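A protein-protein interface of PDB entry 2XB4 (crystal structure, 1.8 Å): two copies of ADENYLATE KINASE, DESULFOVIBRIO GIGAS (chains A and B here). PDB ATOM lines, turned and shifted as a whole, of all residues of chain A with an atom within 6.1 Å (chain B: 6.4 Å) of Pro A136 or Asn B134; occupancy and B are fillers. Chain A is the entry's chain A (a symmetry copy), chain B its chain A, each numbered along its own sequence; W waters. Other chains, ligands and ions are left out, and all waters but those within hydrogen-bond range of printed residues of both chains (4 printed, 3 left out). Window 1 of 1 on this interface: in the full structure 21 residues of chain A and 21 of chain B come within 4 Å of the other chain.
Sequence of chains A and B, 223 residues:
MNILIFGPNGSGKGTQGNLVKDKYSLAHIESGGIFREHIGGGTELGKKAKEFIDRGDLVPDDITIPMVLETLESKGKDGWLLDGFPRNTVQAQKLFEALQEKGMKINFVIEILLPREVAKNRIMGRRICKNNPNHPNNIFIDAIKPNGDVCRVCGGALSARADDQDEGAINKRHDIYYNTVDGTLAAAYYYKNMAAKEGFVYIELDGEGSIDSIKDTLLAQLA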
ATOM      1  N   THR A  15      24.897 -34.536   7.699  1.00  0.00           N
ATOM      2  CA  THR A  15      25.699 -33.722   8.579  1.00  0.00           C
ATOM      3  C   THR A  15      26.351 -34.519   9.684  1.00  0.00           C
ATOM      4  O   THR A  15      27.549 -34.367   9.942  1.00  0.00           O
ATOM      5  CB  THR A  15      24.875 -32.587   9.175  1.00  0.00           C
ATOM      6  OG1 THR A  15      24.314 -31.839   8.101  1.00  0.00           O
ATOM      7  CG2 THR A  15      25.779 -31.642   9.993  1.00  0.00           C
ATOM      8  N   ARG A 127      14.158 -22.305   4.436  1.00  0.00           N
ATOM      9  CA  ARG A 127      14.071 -21.042   3.632  1.00  0.00           C
ATOM     10  C   ARG A 127      15.493 -20.726   3.242  1.00  0.00           C
ATOM     11  O   ARG A 127      16.382 -20.838   4.079  1.00  0.00           O
ATOM     12  CB  ARG A 127      13.487 -19.876   4.437  1.00  0.00           C
ATOM     13  CG  ARG A 127      11.919 -20.134   4.728  1.00  0.00           C
ATOM     14  CD  ARG A 127      11.060 -20.164   3.407  1.00  0.00           C
ATOM     15  NE  ARG A 127       9.623 -20.361   3.679  1.00  0.00           N
ATOM     16  CZ  ARG A 127       9.002 -21.541   3.823  1.00  0.00           C
ATOM     17  NH1 ARG A 127       9.681 -22.695   3.775  1.00  0.00           N
ATOM     18  NH2 ARG A 127       7.690 -21.551   4.102  1.00  0.00           N
ATOM     19  N   PRO A 133      23.554 -19.036   0.373  1.00  0.00           N
ATOM     20  CA  PRO A 133      22.670 -20.208   0.630  1.00  0.00           C
ATOM     21  C   PRO A 133      23.140 -21.029   1.859  1.00  0.00           C
ATOM     22  O   PRO A 133      22.390 -21.843   2.342  1.00  0.00           O
ATOM     23  CB  PRO A 133      22.807 -21.027  -0.682  1.00  0.00           C
ATOM     24  CG  PRO A 133      24.257 -20.723  -1.177  1.00  0.00           C
ATOM     25  CD  PRO A 133      24.402 -19.201  -0.818  1.00  0.00           C
ATOM     26  N   ASN A 134      24.315 -20.733   2.400  1.00  0.00           N
ATOM     27  CA  ASN A 134      24.856 -21.443   3.596  1.00  0.00           C
ATOM     28  C   ASN A 134      24.081 -21.015   4.838  1.00  0.00           C
ATOM     29  O   ASN A 134      24.096 -21.783   5.819  1.00  0.00           O
ATOM     30  CB  ASN A 134      26.343 -21.113   3.933  1.00  0.00           C
ATOM     31  CG  ASN A 134      27.378 -21.535   2.823  1.00  0.00           C
ATOM     32  OD1 ASN A 134      27.082 -22.355   1.942  1.00  0.00           O
ATOM     33  ND2 ASN A 134      28.622 -20.999   2.939  1.00  0.00           N
ATOM     34  N   HIS A 135      23.431 -19.828   4.830  1.00  0.00           N
ATOM     35  CA  HIS A 135      22.814 -19.236   6.097  1.00  0.00           C
ATOM     36  C   HIS A 135      21.565 -20.033   6.548  1.00  0.00           C
ATOM     37  O   HIS A 135      20.573 -19.948   5.881  1.00  0.00           O
ATOM     38  CB  HIS A 135      22.373 -17.754   5.863  1.00  0.00           C
ATOM     39  CG  HIS A 135      23.535 -16.802   5.650  1.00  0.00           C
ATOM     40  ND1 HIS A 135      23.358 -15.497   5.222  1.00  0.00           N
ATOM     41  CD2 HIS A 135      24.866 -16.947   5.874  1.00  0.00           C
ATOM     42  CE1 HIS A 135      24.545 -14.905   5.114  1.00  0.00           C
ATOM     43  NE2 HIS A 135      25.470 -15.756   5.526  1.00  0.00           N
ATOM     44  N   PRO A 136      21.626 -20.783   7.677  1.00  0.00           N
ATOM     45  CA  PRO A 136      20.464 -21.672   7.953  1.00  0.00           C
ATOM     46  C   PRO A 136      19.229 -20.904   8.434  1.00  0.00           C
ATOM     47  O   PRO A 136      19.327 -20.072   9.357  1.00  0.00           O
ATOM     48  CB  PRO A 136      21.000 -22.658   9.054  1.00  0.00           C
ATOM     49  CG  PRO A 136      22.512 -22.627   8.920  1.00  0.00           C
ATOM     50  CD  PRO A 136      22.772 -21.088   8.557  1.00  0.00           C
ATOM     51  N   ASN A 137      18.080 -21.146   7.802  1.00  0.00           N
ATOM     52  CA  ASN A 137      16.795 -20.540   8.216  1.00  0.00           C
ATOM     53  C   ASN A 137      15.743 -21.627   8.095  1.00  0.00           C
ATOM     54  O   ASN A 137      15.699 -22.309   7.077  1.00  0.00           O
ATOM     55  CB  ASN A 137      16.347 -19.374   7.305  1.00  0.00           C
ATOM     56  CG  ASN A 137      17.277 -18.088   7.461  1.00  0.00           C
ATOM     57  OD1 ASN A 137      18.350 -17.972   6.781  1.00  0.00           O
ATOM     58  ND2 ASN A 137      16.880 -17.153   8.280  1.00  0.00           N
ATOM     59  N   ASN A 138      14.885 -21.746   9.107  1.00  0.00           N
ATOM     60  CA  ASN A 138      13.875 -22.763   9.039  1.00  0.00           C
ATOM     61  C   ASN A 138      12.702 -22.297   9.899  1.00  0.00           C
ATOM     62  O   ASN A 138      12.855 -22.152  11.123  1.00  0.00           O
ATOM     63  CB  ASN A 138      14.403 -24.134   9.511  1.00  0.00           C
ATOM     64  CG  ASN A 138      13.481 -25.271   9.103  1.00  0.00           C
ATOM     65  OD1 ASN A 138      12.248 -25.260   9.458  1.00  0.00           O
ATOM     66  ND2 ASN A 138      14.026 -26.251   8.350  1.00  0.00           N
ATOM     67  N   ILE A 144      16.755 -21.569  14.620  1.00  0.00           N
ATOM     68  CA  ILE A 144      17.129 -20.894  13.367  1.00  0.00           C
ATOM     69  C   ILE A 144      15.922 -20.337  12.580  1.00  0.00           C
ATOM     70  O   ILE A 144      15.977 -20.259  11.359  1.00  0.00           O
ATOM     71  CB  ILE A 144      17.952 -21.833  12.433  1.00  0.00           C
ATOM     72  CG1 ILE A 144      17.198 -23.152  12.209  1.00  0.00           C
ATOM     73  CG2 ILE A 144      19.294 -22.135  13.054  1.00  0.00           C
ATOM     74  CD1 ILE A 144      17.666 -23.987  10.978  1.00  0.00           C
ATOM     75  N   LYS A 145      14.845 -19.917  13.270  1.00  0.00           N
ATOM     76  CA  LYS A 145      13.698 -19.227  12.697  1.00  0.00           C
ATOM     77  C   LYS A 145      14.170 -17.999  12.009  1.00  0.00           C
ATOM     78  O   LYS A 145      15.124 -17.362  12.510  1.00  0.00           O
ATOM     79  CB  LYS A 145      12.810 -18.612  13.818  1.00  0.00           C
ATOM     80  CG  LYS A 145      12.019 -19.493  14.600  1.00  0.00           C
ATOM     81  CD  LYS A 145      11.229 -18.592  15.667  1.00  0.00           C
ATOM     82  CE  LYS A 145      12.069 -17.493  16.492  1.00  0.00           C
ATOM     83  NZ  LYS A 145      11.317 -17.124  17.792  1.00  0.00           N
ATOM     84  N   CYS A 151      16.398 -13.278   6.145  1.00  0.00           N
ATOM     85  CA  CYS A 151      17.460 -14.132   6.701  1.00  0.00           C
ATOM     86  C   CYS A 151      17.887 -13.676   8.099  1.00  0.00           C
ATOM     87  O   CYS A 151      18.169 -12.491   8.272  1.00  0.00           O
ATOM     88  CB  CYS A 151      18.682 -14.105   5.740  1.00  0.00           C
ATOM     89  SG  CYS A 151      20.035 -15.121   6.404  1.00  0.00           S
ATOM     90  N   ARG A 152      17.940 -14.592   9.090  1.00  0.00           N
ATOM     91  CA  ARG A 152      18.305 -14.257  10.474  1.00  0.00           C
ATOM     92  C   ARG A 152      19.799 -13.956  10.623  1.00  0.00           C
ATOM     93  O   ARG A 152      20.230 -13.457  11.658  1.00  0.00           O
ATOM     94  CB  ARG A 152      17.979 -15.451  11.383  1.00  0.00           C
ATOM     95  CG  ARG A 152      18.848 -16.709  10.975  1.00  0.00           C
ATOM     96  CD  ARG A 152      18.469 -17.942  11.767  1.00  0.00           C
ATOM     97  NE  ARG A 152      18.318 -17.610  13.177  1.00  0.00           N
ATOM     98  CZ  ARG A 152      19.337 -17.632  14.024  1.00  0.00           C
ATOM     99  NH1 ARG A 152      20.557 -17.976  13.523  1.00  0.00           N
ATOM    100  NH2 ARG A 152      19.144 -17.304  15.334  1.00  0.00           N
ATOM    101  N   VAL A 153      20.606 -14.294   9.613  1.00  0.00           N
ATOM    102  CA  VAL A 153      22.069 -14.034   9.679  1.00  0.00           C
ATOM    103  C   VAL A 153      22.368 -12.678   9.071  1.00  0.00           C
ATOM    104  O   VAL A 153      23.117 -11.906   9.650  1.00  0.00           O
ATOM    105  CB  VAL A 153      22.876 -15.099   8.846  1.00  0.00           C
ATOM    106  CG1 VAL A 153      24.411 -14.822   8.934  1.00  0.00           C
ATOM    107  CG2 VAL A 153      22.616 -16.517   9.338  1.00  0.00           C
ATOM    108  N   ILE A 211      22.363 -29.308  16.551  1.00  0.00           N
ATOM    109  CA  ILE A 211      23.447 -29.990  15.762  1.00  0.00           C
ATOM    110  C   ILE A 211      24.600 -30.354  16.743  1.00  0.00           C
ATOM    111  O   ILE A 211      25.090 -31.495  16.719  1.00  0.00           O
ATOM    112  CB  ILE A 211      24.008 -29.179  14.452  1.00  0.00           C
ATOM    113  CG1 ILE A 211      22.969 -29.031  13.316  1.00  0.00           C
ATOM    114  CG2 ILE A 211      25.349 -29.800  13.884  1.00  0.00           C
ATOM    115  CD1 ILE A 211      23.365 -27.971  12.224  1.00  0.00           C
ATOM    116  N   ILE B 128      24.213 -26.099  -4.675  1.00  0.00           N
ATOM    117  CA  ILE B 128      23.339 -26.354  -3.518  1.00  0.00           C
ATOM    118  C   ILE B 128      23.044 -27.837  -3.477  1.00  0.00           C
ATOM    119  O   ILE B 128      22.680 -28.439  -4.496  1.00  0.00           O
ATOM    120  CB  ILE B 128      21.982 -25.639  -3.699  1.00  0.00           C
ATOM    121  CG1 ILE B 128      22.165 -24.159  -3.976  1.00  0.00           C
ATOM    122  CG2 ILE B 128      21.072 -25.850  -2.421  1.00  0.00           C
ATOM    123  CD1 ILE B 128      23.349 -23.535  -3.221  1.00  0.00           C
ATOM    124  N   CYS B 129      23.184 -28.441  -2.283  1.00  0.00           N
ATOM    125  CA  CYS B 129      22.814 -29.820  -2.072  1.00  0.00           C
ATOM    126  C   CYS B 129      21.302 -30.029  -1.992  1.00  0.00           C
ATOM    127  O   CYS B 129      20.590 -29.355  -1.213  1.00  0.00           O
ATOM    128  CB  CYS B 129      23.495 -30.298  -0.761  1.00  0.00           C
ATOM    129  SG  CYS B 129      23.062 -32.032  -0.251  1.00  0.00           S
ATOM    130  N   ASN B 132      20.314 -31.239   1.744  1.00  0.00           N
ATOM    131  CA  ASN B 132      20.325 -30.238   2.816  1.00  0.00           C
ATOM    132  C   ASN B 132      21.017 -28.968   2.323  1.00  0.00           C
ATOM    133  O   ASN B 132      22.228 -28.982   2.067  1.00  0.00           O
ATOM    134  CB  ASN B 132      21.100 -30.808   4.022  1.00  0.00           C
ATOM    135  CG  ASN B 132      21.029 -29.877   5.279  1.00  0.00           C
ATOM    136  OD1 ASN B 132      20.928 -28.665   5.171  1.00  0.00           O
ATOM    137  ND2 ASN B 132      21.138 -30.479   6.464  1.00  0.00           N
ATOM    138  N   PRO B 133      20.263 -27.863   2.181  1.00  0.00           N
ATOM    139  CA  PRO B 133      20.852 -26.664   1.521  1.00  0.00           C
ATOM    140  C   PRO B 133      21.932 -25.988   2.405  1.00  0.00           C
ATOM    141  O   PRO B 133      22.671 -25.173   1.907  1.00  0.00           O
ATOM    142  CB  PRO B 133      19.617 -25.742   1.335  1.00  0.00           C
ATOM    143  CG  PRO B 133      18.688 -26.094   2.541  1.00  0.00           C
ATOM    144  CD  PRO B 133      18.885 -27.649   2.649  1.00  0.00           C
ATOM    145  N   ASN B 134      22.072 -26.407   3.656  1.00  0.00           N
ATOM    146  CA  ASN B 134      23.092 -25.843   4.588  1.00  0.00           C
ATOM    147  C   ASN B 134      24.480 -26.328   4.180  1.00  0.00           C
ATOM    148  O   ASN B 134      25.458 -25.653   4.553  1.00  0.00           O
ATOM    149  CB  ASN B 134      22.942 -26.298   6.072  1.00  0.00           C
ATOM    150  CG  ASN B 134      21.601 -25.847   6.765  1.00  0.00           C
ATOM    151  OD1 ASN B 134      20.906 -24.935   6.296  1.00  0.00           O
ATOM    152  ND2 ASN B 134      21.301 -26.472   7.935  1.00  0.00           N
ATOM    153  N   HIS B 135      24.591 -27.465   3.454  1.00  0.00           N
ATOM    154  CA  HIS B 135      25.944 -28.126   3.190  1.00  0.00           C
ATOM    155  C   HIS B 135      26.802 -27.292   2.206  1.00  0.00           C
ATOM    156  O   HIS B 135      26.463 -27.253   1.058  1.00  0.00           O
ATOM    157  CB  HIS B 135      25.758 -29.550   2.569  1.00  0.00           C
ATOM    158  CG  HIS B 135      25.142 -30.552   3.527  1.00  0.00           C
ATOM    159  ND1 HIS B 135      24.703 -31.800   3.115  1.00  0.00           N
ATOM    160  CD2 HIS B 135      24.962 -30.515   4.872  1.00  0.00           C
ATOM    161  CE1 HIS B 135      24.203 -32.456   4.160  1.00  0.00           C
ATOM    162  NE2 HIS B 135      24.371 -31.708   5.237  1.00  0.00           N
ATOM    163  N   PRO B 136      27.907 -26.652   2.666  1.00  0.00           N
ATOM    164  CA  PRO B 136      28.579 -25.717   1.721  1.00  0.00           C
ATOM    165  C   PRO B 136      29.359 -26.442   0.621  1.00  0.00           C
ATOM    166  O   PRO B 136      30.153 -27.358   0.914  1.00  0.00           O
ATOM    167  CB  PRO B 136      29.527 -24.870   2.645  1.00  0.00           C
ATOM    168  CG  PRO B 136      28.942 -24.987   4.040  1.00  0.00           C
ATOM    169  CD  PRO B 136      28.417 -26.502   4.043  1.00  0.00           C
ATOM    170  N   ASN B 137      29.121 -26.071  -0.637  1.00  0.00           N
ATOM    171  CA  ASN B 137      29.864 -26.626  -1.791  1.00  0.00           C
ATOM    172  C   ASN B 137      30.138 -25.466  -2.730  1.00  0.00           C
ATOM    173  O   ASN B 137      29.227 -24.694  -3.013  1.00  0.00           O
ATOM    174  CB  ASN B 137      29.056 -27.674  -2.590  1.00  0.00           C
ATOM    175  CG  ASN B 137      28.839 -29.027  -1.774  1.00  0.00           C
ATOM    176  OD1 ASN B 137      27.861 -29.151  -0.965  1.00  0.00           O
ATOM    177  ND2 ASN B 137      29.677 -30.003  -1.992  1.00  0.00           N
HETATM  178  O   HOH W   1      20.923 -23.340   4.331  1.00  0.00           O
HETATM  179  O   HOH W   2      25.104 -23.766   1.234  1.00  0.00           O
HETATM  180  O   HOH W   3      23.368 -28.671   8.651  1.00  0.00           O
HETATM  181  O   HOH W   4      22.138 -30.781   9.696  1.00  0.00           O
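The side-chain hydroxyl (OG1) of Thr A15 sits at hydrogen-bond distance from a ring nitrogen (NE2) of His B135 (2.9 Å).
The backbone carbonyl oxygen (O) of Pro A133 sits close to the backbone carbonyl oxygen (O) of Pro B133, 3.4 Å away.
O of His B135 lies close to OD1 of Asn B137 (3.1 Å).
The backbone NH (N) of Asn B132 lies close to the side-chain sulfur (SG) of Cys B129 (3.5 Å).
The side-chain amide oxygen (OD1) of Asn B132 is in hydrogen-bond range of the backbone NH (N) of Asn B134, 3.0 Å away.
Thr A15 touches Asn B132.
Pro A133 touches Ile B128 (CG to CD1, 3.6 Å).
OD1 of Asn A134 touches CB of Pro B136, 3.6 Å away.
Asn B134 touches Pro A136.
Asn B134 touches one residue of chain A.
Of the printed residues of chain A, Asn B132 touches Thr A15 (3.8 Å).
Printed residues of chain B within 4 Å of Thr A15: Asn B132 and His B135.
Asn A137 touches none of the printed residues of chain B.
His A135 touches none of the printed residues of chain B.
The nearest residue of chain A that does not touch Asn B134 is Asn A134 (4.3 Å).
Printed residues of chain B that touch a printed residue of chain A: Ile B128, Asn B132, Pro B133, Asn B134, His B135 and Pro B136.
Hydrophobic or aromatic side chains of chain B that line the printed part of chain A: Ile B128, His B135 and Pro B136.
Hydrophobic or aromatic side chains of chain A that line the printed part of chain B: Pro A133 and Pro A136.
Among the printed residues, 6 pairs touch across the chains.
Among the printed residues, no Asp or Glu carboxylate lies within 4 Å of a Lys or Arg side-chain nitrogen of the other chain.
Pro A133 touches its own counterpart, Pro B133.
Asn A134 touches Pro B136, and with the chains exchanged Pro A136 touches Asn B134.
Of the 6 pairs that touch across the chains among the printed residues, 3 have their exchanged pair printed and touching as well.
Water W2 lies within hydrogen-bond range of the side-chain amide oxygen of Asn A134 (2.5 Å) and the backbone carbonyl oxygen of Pro B133 (2.9 Å).
Water W1 bridges OD1 of Asn B134 (2.5 Å) and O of Pro A133 (2.9 Å).
Water W4 lies within hydrogen-bond range of the side-chain hydroxyl (OG1) of Thr A15 (2.9 Å) and the side-chain amide nitrogen (ND2) of Asn B132 (3.4 Å).
Water W3 lies within hydrogen-bond range of ND2 of Asn B134 (3.1 Å) and OG1 of Thr A15 (3.4 Å).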
